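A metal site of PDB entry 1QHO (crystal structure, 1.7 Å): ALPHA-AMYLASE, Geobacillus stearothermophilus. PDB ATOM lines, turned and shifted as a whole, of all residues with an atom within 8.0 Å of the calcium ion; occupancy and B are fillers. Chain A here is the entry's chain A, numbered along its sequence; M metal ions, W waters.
N of Gly 53 sits at hydrogen-bond distance from OD1 of Asp 50, 2.8 Å away.
The side-chain carboxylate (OD1) of Asp 50 lies within hydrogen-bond range of the backbone NH (N) of Gly 22.
ND2 of Asn 27 is in hydrogen-bond range of OH of Tyr 36 (3.2 Å).
O of Tyr 20 sits at hydrogen-bond distance from N of Asp 50 (3.0 Å).
The side-chain carboxylate (OD1) of Asp 17 lies within hydrogen-bond range of the backbone NH (N) of Gly 48, 2.9 Å away.
OD1 of Asn 27 lies close to O of Thr 24 (3.4 Å).
The side-chain hydroxyl of Thr 25 is in hydrogen-bond range of the side-chain carboxylate of Asp 23 (2.7 Å).
A ring nitrogen (NE2) of His 103 sits close to the backbone carbonyl oxygen of Asn 27, at 3.5 Å.
Six residues have an atom within 4 Å of the calcium ion: Asp 21, Asp 23, Asn 26, Asn 27, Gly 48 and Asp 50.
The calcium ion is bound by the side-chain amide oxygen of Asn 27, the side-chain carboxylate of Asp 50, the side-chain amide oxygen of Asn 26, the backbone carbonyl oxygen of Gly 48, the side-chain carboxylate of Asp 21, the backbone carbonyl oxygen of Asp 23 and water W1.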
ATOM      1  N   ILE A  16      -4.927  14.304 -25.754  1.00  0.00           N
ATOM      2  CA  ILE A  16      -5.390  15.669 -25.594  1.00  0.00           C
ATOM      3  C   ILE A  16      -6.387  16.150 -26.648  1.00  0.00           C
ATOM      4  O   ILE A  16      -7.444  16.696 -26.278  1.00  0.00           O
ATOM      5  CB  ILE A  16      -4.202  16.643 -25.541  1.00  0.00           C
ATOM      6  CG1 ILE A  16      -3.395  16.354 -24.243  1.00  0.00           C
ATOM      7  CG2 ILE A  16      -4.650  18.099 -25.537  1.00  0.00           C
ATOM      8  CD1 ILE A  16      -2.011  16.994 -24.311  1.00  0.00           C
ATOM      9  N   ASP A  17      -6.072  15.970 -27.927  1.00  0.00           N
ATOM     10  CA  ASP A  17      -6.974  16.457 -28.966  1.00  0.00           C
ATOM     11  C   ASP A  17      -8.356  15.825 -28.952  1.00  0.00           C
ATOM     12  O   ASP A  17      -9.306  16.401 -29.510  1.00  0.00           O
ATOM     13  CB  ASP A  17      -6.305  16.153 -30.329  1.00  0.00           C
ATOM     14  CG  ASP A  17      -7.144  16.706 -31.487  1.00  0.00           C
ATOM     15  OD1 ASP A  17      -7.240  17.951 -31.556  1.00  0.00           O
ATOM     16  OD2 ASP A  17      -7.673  15.917 -32.285  1.00  0.00           O
ATOM     17  N   TYR A  20     -11.276  17.033 -24.402  1.00  0.00           N
ATOM     18  CA  TYR A  20     -12.235  18.122 -24.241  1.00  0.00           C
ATOM     19  C   TYR A  20     -11.696  19.425 -24.820  1.00  0.00           C
ATOM     20  O   TYR A  20     -10.574  19.825 -24.534  1.00  0.00           O
ATOM     21  CB  TYR A  20     -12.613  18.301 -22.758  1.00  0.00           C
ATOM     22  CG  TYR A  20     -13.833  19.181 -22.580  1.00  0.00           C
ATOM     23  CD1 TYR A  20     -15.087  18.711 -22.952  1.00  0.00           C
ATOM     24  CD2 TYR A  20     -13.738  20.452 -22.030  1.00  0.00           C
ATOM     25  CE1 TYR A  20     -16.220  19.495 -22.783  1.00  0.00           C
ATOM     26  CE2 TYR A  20     -14.871  21.236 -21.861  1.00  0.00           C
ATOM     27  CZ  TYR A  20     -16.096  20.756 -22.247  1.00  0.00           C
ATOM     28  OH  TYR A  20     -17.230  21.531 -22.088  1.00  0.00           O
ATOM     29  N   ASP A  21     -12.533  20.053 -25.631  1.00  0.00           N
ATOM     30  CA  ASP A  21     -12.175  21.334 -26.278  1.00  0.00           C
ATOM     31  C   ASP A  21     -12.553  22.445 -25.295  1.00  0.00           C
ATOM     32  O   ASP A  21     -13.687  22.919 -25.269  1.00  0.00           O
ATOM     33  CB  ASP A  21     -12.945  21.417 -27.587  1.00  0.00           C
ATOM     34  CG  ASP A  21     -12.659  22.626 -28.438  1.00  0.00           C
ATOM     35  OD1 ASP A  21     -11.850  23.447 -27.983  1.00  0.00           O
ATOM     36  OD2 ASP A  21     -13.238  22.794 -29.528  1.00  0.00           O
ATOM     37  N   GLY A  22     -11.594  22.859 -24.471  1.00  0.00           N
ATOM     38  CA  GLY A  22     -11.856  23.867 -23.447  1.00  0.00           C
ATOM     39  C   GLY A  22     -11.664  25.295 -23.953  1.00  0.00           C
ATOM     40  O   GLY A  22     -12.006  26.274 -23.272  1.00  0.00           O
ATOM     41  N   ASP A  23     -11.110  25.436 -25.148  1.00  0.00           N
ATOM     42  CA  ASP A  23     -10.853  26.758 -25.729  1.00  0.00           C
ATOM     43  C   ASP A  23     -11.076  26.636 -27.227  1.00  0.00           C
ATOM     44  O   ASP A  23     -10.148  26.181 -27.890  1.00  0.00           O
ATOM     45  CB  ASP A  23      -9.422  27.191 -25.433  1.00  0.00           C
ATOM     46  CG  ASP A  23      -9.114  28.594 -25.966  1.00  0.00           C
ATOM     47  OD1 ASP A  23      -9.973  29.167 -26.661  1.00  0.00           O
ATOM     48  OD2 ASP A  23      -8.012  29.082 -25.698  1.00  0.00           O
ATOM     49  N   THR A  24     -12.189  27.055 -27.794  1.00  0.00           N
ATOM     50  CA  THR A  24     -12.364  26.886 -29.247  1.00  0.00           C
ATOM     51  C   THR A  24     -11.497  27.820 -30.069  1.00  0.00           C
ATOM     52  O   THR A  24     -11.346  27.583 -31.276  1.00  0.00           O
ATOM     53  CB  THR A  24     -13.843  27.085 -29.636  1.00  0.00           C
ATOM     54  OG1 THR A  24     -14.217  28.435 -29.285  1.00  0.00           O
ATOM     55  CG2 THR A  24     -14.735  26.094 -28.903  1.00  0.00           C
ATOM     56  N   THR A  25     -10.844  28.818 -29.482  1.00  0.00           N
ATOM     57  CA  THR A  25     -10.059  29.795 -30.213  1.00  0.00           C
ATOM     58  C   THR A  25      -8.720  29.258 -30.690  1.00  0.00           C
ATOM     59  O   THR A  25      -8.100  29.938 -31.524  1.00  0.00           O
ATOM     60  CB  THR A  25      -9.791  31.108 -29.453  1.00  0.00           C
ATOM     61  OG1 THR A  25      -8.863  30.942 -28.386  1.00  0.00           O
ATOM     62  CG2 THR A  25     -11.100  31.677 -28.912  1.00  0.00           C
ATOM     63  N   ASN A  26      -8.270  28.100 -30.193  1.00  0.00           N
ATOM     64  CA  ASN A  26      -6.990  27.581 -30.690  1.00  0.00           C
ATOM     65  C   ASN A  26      -7.228  26.393 -31.609  1.00  0.00           C
ATOM     66  O   ASN A  26      -6.296  25.664 -31.940  1.00  0.00           O
ATOM     67  CB  ASN A  26      -6.077  27.273 -29.508  1.00  0.00           C
ATOM     68  CG  ASN A  26      -6.631  26.253 -28.544  1.00  0.00           C
ATOM     69  OD1 ASN A  26      -7.525  25.526 -28.960  1.00  0.00           O
ATOM     70  ND2 ASN A  26      -6.176  26.141 -27.303  1.00  0.00           N
ATOM     71  N   ASN A  27      -8.462  26.208 -32.090  1.00  0.00           N
ATOM     72  CA  ASN A  27      -8.778  25.069 -32.941  1.00  0.00           C
ATOM     73  C   ASN A  27      -8.112  25.096 -34.310  1.00  0.00           C
ATOM     74  O   ASN A  27      -7.784  24.044 -34.861  1.00  0.00           O
ATOM     75  CB  ASN A  27     -10.297  24.953 -33.185  1.00  0.00           C
ATOM     76  CG  ASN A  27     -11.034  24.437 -31.986  1.00  0.00           C
ATOM     77  OD1 ASN A  27     -10.372  24.334 -30.960  1.00  0.00           O
ATOM     78  ND2 ASN A  27     -12.313  24.099 -31.974  1.00  0.00           N
ATOM     79  N   ASN A  28      -7.878  26.284 -34.864  1.00  0.00           N
ATOM     80  CA  ASN A  28      -7.305  26.362 -36.213  1.00  0.00           C
ATOM     81  C   ASN A  28      -6.440  27.602 -36.325  1.00  0.00           C
ATOM     82  O   ASN A  28      -6.794  28.592 -36.985  1.00  0.00           O
ATOM     83  CB  ASN A  28      -8.499  26.435 -37.167  1.00  0.00           C
ATOM     84  CG  ASN A  28      -8.164  26.160 -38.619  1.00  0.00           C
ATOM     85  OD1 ASN A  28      -7.113  25.632 -38.957  1.00  0.00           O
ATOM     86  ND2 ASN A  28      -9.116  26.503 -39.500  1.00  0.00           N
ATOM     87  N   TYR A  36      -7.641  21.355 -38.930  1.00  0.00           N
ATOM     88  CA  TYR A  36      -8.769  21.167 -38.038  1.00  0.00           C
ATOM     89  C   TYR A  36     -10.016  20.662 -38.757  1.00  0.00           C
ATOM     90  O   TYR A  36     -10.374  21.159 -39.824  1.00  0.00           O
ATOM     91  CB  TYR A  36      -9.071  22.523 -37.387  1.00  0.00           C
ATOM     92  CG  TYR A  36     -10.362  22.624 -36.601  1.00  0.00           C
ATOM     93  CD1 TYR A  36     -10.626  21.796 -35.520  1.00  0.00           C
ATOM     94  CD2 TYR A  36     -11.317  23.568 -36.971  1.00  0.00           C
ATOM     95  CE1 TYR A  36     -11.804  21.932 -34.802  1.00  0.00           C
ATOM     96  CE2 TYR A  36     -12.489  23.697 -36.257  1.00  0.00           C
ATOM     97  CZ  TYR A  36     -12.729  22.876 -35.175  1.00  0.00           C
ATOM     98  OH  TYR A  36     -13.916  23.000 -34.474  1.00  0.00           O
ATOM     99  N   TRP A  47      -9.223  17.550 -33.840  1.00  0.00           N
ATOM    100  CA  TRP A  47     -10.635  17.718 -33.524  1.00  0.00           C
ATOM    101  C   TRP A  47     -10.868  18.837 -32.504  1.00  0.00           C
ATOM    102  O   TRP A  47     -12.007  19.270 -32.292  1.00  0.00           O
ATOM    103  CB  TRP A  47     -11.296  16.414 -33.074  1.00  0.00           C
ATOM    104  CG  TRP A  47     -11.452  15.419 -34.195  1.00  0.00           C
ATOM    105  CD1 TRP A  47     -11.144  15.572 -35.510  1.00  0.00           C
ATOM    106  CD2 TRP A  47     -12.051  14.126 -34.079  1.00  0.00           C
ATOM    107  NE1 TRP A  47     -11.435  14.432 -36.212  1.00  0.00           N
ATOM    108  CE2 TRP A  47     -11.998  13.527 -35.357  1.00  0.00           C
ATOM    109  CE3 TRP A  47     -12.558  13.379 -33.010  1.00  0.00           C
ATOM    110  CZ2 TRP A  47     -12.488  12.246 -35.600  1.00  0.00           C
ATOM    111  CZ3 TRP A  47     -13.045  12.115 -33.249  1.00  0.00           C
ATOM    112  CH2 TRP A  47     -13.002  11.556 -34.532  1.00  0.00           C
ATOM    113  N   GLY A  48      -9.802  19.290 -31.856  1.00  0.00           N
ATOM    114  CA  GLY A  48      -9.951  20.461 -30.991  1.00  0.00           C
ATOM    115  C   GLY A  48      -9.748  20.285 -29.523  1.00  0.00           C
ATOM    116  O   GLY A  48      -9.780  21.316 -28.811  1.00  0.00           O
ATOM    117  N   GLY A  49      -9.528  19.116 -28.977  1.00  0.00           N
ATOM    118  CA  GLY A  49      -9.293  18.998 -27.524  1.00  0.00           C
ATOM    119  C   GLY A  49      -8.006  19.713 -27.161  1.00  0.00           C
ATOM    120  O   GLY A  49      -7.038  19.704 -27.933  1.00  0.00           O
ATOM    121  N   ASP A  50      -7.922  20.225 -25.923  1.00  0.00           N
ATOM    122  CA  ASP A  50      -6.706  20.971 -25.571  1.00  0.00           C
ATOM    123  C   ASP A  50      -6.392  20.924 -24.083  1.00  0.00           C
ATOM    124  O   ASP A  50      -7.062  20.243 -23.319  1.00  0.00           O
ATOM    125  CB  ASP A  50      -6.893  22.416 -26.059  1.00  0.00           C
ATOM    126  CG  ASP A  50      -8.237  22.958 -25.595  1.00  0.00           C
ATOM    127  OD1 ASP A  50      -8.712  22.637 -24.504  1.00  0.00           O
ATOM    128  OD2 ASP A  50      -8.902  23.707 -26.309  1.00  0.00           O
ATOM    129  N   LEU A  51      -5.316  21.600 -23.696  1.00  0.00           N
ATOM    130  CA  LEU A  51      -4.876  21.567 -22.297  1.00  0.00           C
ATOM    131  C   LEU A  51      -5.879  22.240 -21.376  1.00  0.00           C
ATOM    132  O   LEU A  51      -6.123  21.771 -20.261  1.00  0.00           O
ATOM    133  CB  LEU A  51      -3.511  22.250 -22.138  1.00  0.00           C
ATOM    134  CG  LEU A  51      -2.372  21.517 -22.868  1.00  0.00           C
ATOM    135  CD1 LEU A  51      -1.140  22.397 -22.887  1.00  0.00           C
ATOM    136  CD2 LEU A  51      -2.087  20.167 -22.218  1.00  0.00           C
ATOM    137  N   GLU A  52      -6.497  23.326 -21.852  1.00  0.00           N
ATOM    138  CA  GLU A  52      -7.539  23.975 -21.019  1.00  0.00           C
ATOM    139  C   GLU A  52      -8.754  23.083 -20.822  1.00  0.00           C
ATOM    140  O   GLU A  52      -9.374  23.083 -19.744  1.00  0.00           O
ATOM    141  CB  GLU A  52      -7.847  25.328 -21.661  1.00  0.00           C
ATOM    142  CG  GLU A  52      -8.984  26.096 -21.045  1.00  0.00           C
ATOM    143  CD  GLU A  52      -8.827  26.413 -19.560  1.00  0.00           C
ATOM    144  OE1 GLU A  52      -7.711  26.427 -19.023  1.00  0.00           O
ATOM    145  OE2 GLU A  52      -9.900  26.660 -18.986  1.00  0.00           O
ATOM    146  N   GLY A  53      -9.075  22.215 -21.777  1.00  0.00           N
ATOM    147  CA  GLY A  53     -10.160  21.242 -21.661  1.00  0.00           C
ATOM    148  C   GLY A  53      -9.832  20.228 -20.574  1.00  0.00           C
ATOM    149  O   GLY A  53     -10.717  19.878 -19.779  1.00  0.00           O
ATOM    150  N   GLU A 102       0.513  24.672 -30.494  1.00  0.00           N
ATOM    151  CA  GLU A 102      -0.422  25.803 -30.493  1.00  0.00           C
ATOM    152  C   GLU A 102      -1.884  25.417 -30.517  1.00  0.00           C
ATOM    153  O   GLU A 102      -2.718  26.154 -29.967  1.00  0.00           O
ATOM    154  CB  GLU A 102      -0.094  26.795 -31.628  1.00  0.00           C
ATOM    155  CG  GLU A 102      -0.396  26.295 -33.035  1.00  0.00           C
ATOM    156  CD  GLU A 102       0.646  25.364 -33.576  1.00  0.00           C
ATOM    157  OE1 GLU A 102       1.717  25.145 -32.974  1.00  0.00           O
ATOM    158  OE2 GLU A 102       0.401  24.805 -34.684  1.00  0.00           O
ATOM    159  N   HIS A 103      -2.268  24.253 -31.068  1.00  0.00           N
ATOM    160  CA  HIS A 103      -3.636  23.788 -30.956  1.00  0.00           C
ATOM    161  C   HIS A 103      -4.006  23.482 -29.512  1.00  0.00           C
ATOM    162  O   HIS A 103      -5.197  23.482 -29.182  1.00  0.00           O
ATOM    163  CB  HIS A 103      -3.849  22.489 -31.771  1.00  0.00           C
ATOM    164  CG  HIS A 103      -3.919  22.693 -33.247  1.00  0.00           C
ATOM    165  ND1 HIS A 103      -2.791  22.753 -34.047  1.00  0.00           N
ATOM    166  CD2 HIS A 103      -4.977  22.853 -34.063  1.00  0.00           C
ATOM    167  CE1 HIS A 103      -3.172  22.941 -35.312  1.00  0.00           C
ATOM    168  NE2 HIS A 103      -4.492  23.000 -35.342  1.00  0.00           N
ATOM    169  N   PHE A 104      -3.024  23.188 -28.658  1.00  0.00           N
ATOM    170  CA  PHE A 104      -3.310  22.807 -27.277  1.00  0.00           C
ATOM    171  C   PHE A 104      -3.192  23.926 -26.251  1.00  0.00           C
ATOM    172  O   PHE A 104      -3.794  23.790 -25.179  1.00  0.00           O
ATOM    173  CB  PHE A 104      -2.413  21.623 -26.872  1.00  0.00           C
ATOM    174  CG  PHE A 104      -2.527  20.384 -27.719  1.00  0.00           C
ATOM    175  CD1 PHE A 104      -3.593  20.145 -28.564  1.00  0.00           C
ATOM    176  CD2 PHE A 104      -1.544  19.407 -27.623  1.00  0.00           C
ATOM    177  CE1 PHE A 104      -3.687  18.998 -29.332  1.00  0.00           C
ATOM    178  CE2 PHE A 104      -1.619  18.251 -28.378  1.00  0.00           C
ATOM    179  CZ  PHE A 104      -2.692  18.038 -29.243  1.00  0.00           C
ATOM    180  N   GLY A 105      -2.462  24.987 -26.571  1.00  0.00           N
ATOM    181  CA  GLY A 105      -2.313  26.113 -25.648  1.00  0.00           C
ATOM    182  C   GLY A 105      -0.896  26.668 -25.795  1.00  0.00           C
ATOM    183  O   GLY A 105      -0.269  26.502 -26.852  1.00  0.00           O
HETATM  184 CA    CA M   1      -9.428  23.842 -28.746  1.00  0.00          CA
HETATM  185  O   HOH W   1      -7.514  22.832 -30.253  1.00  0.00           O
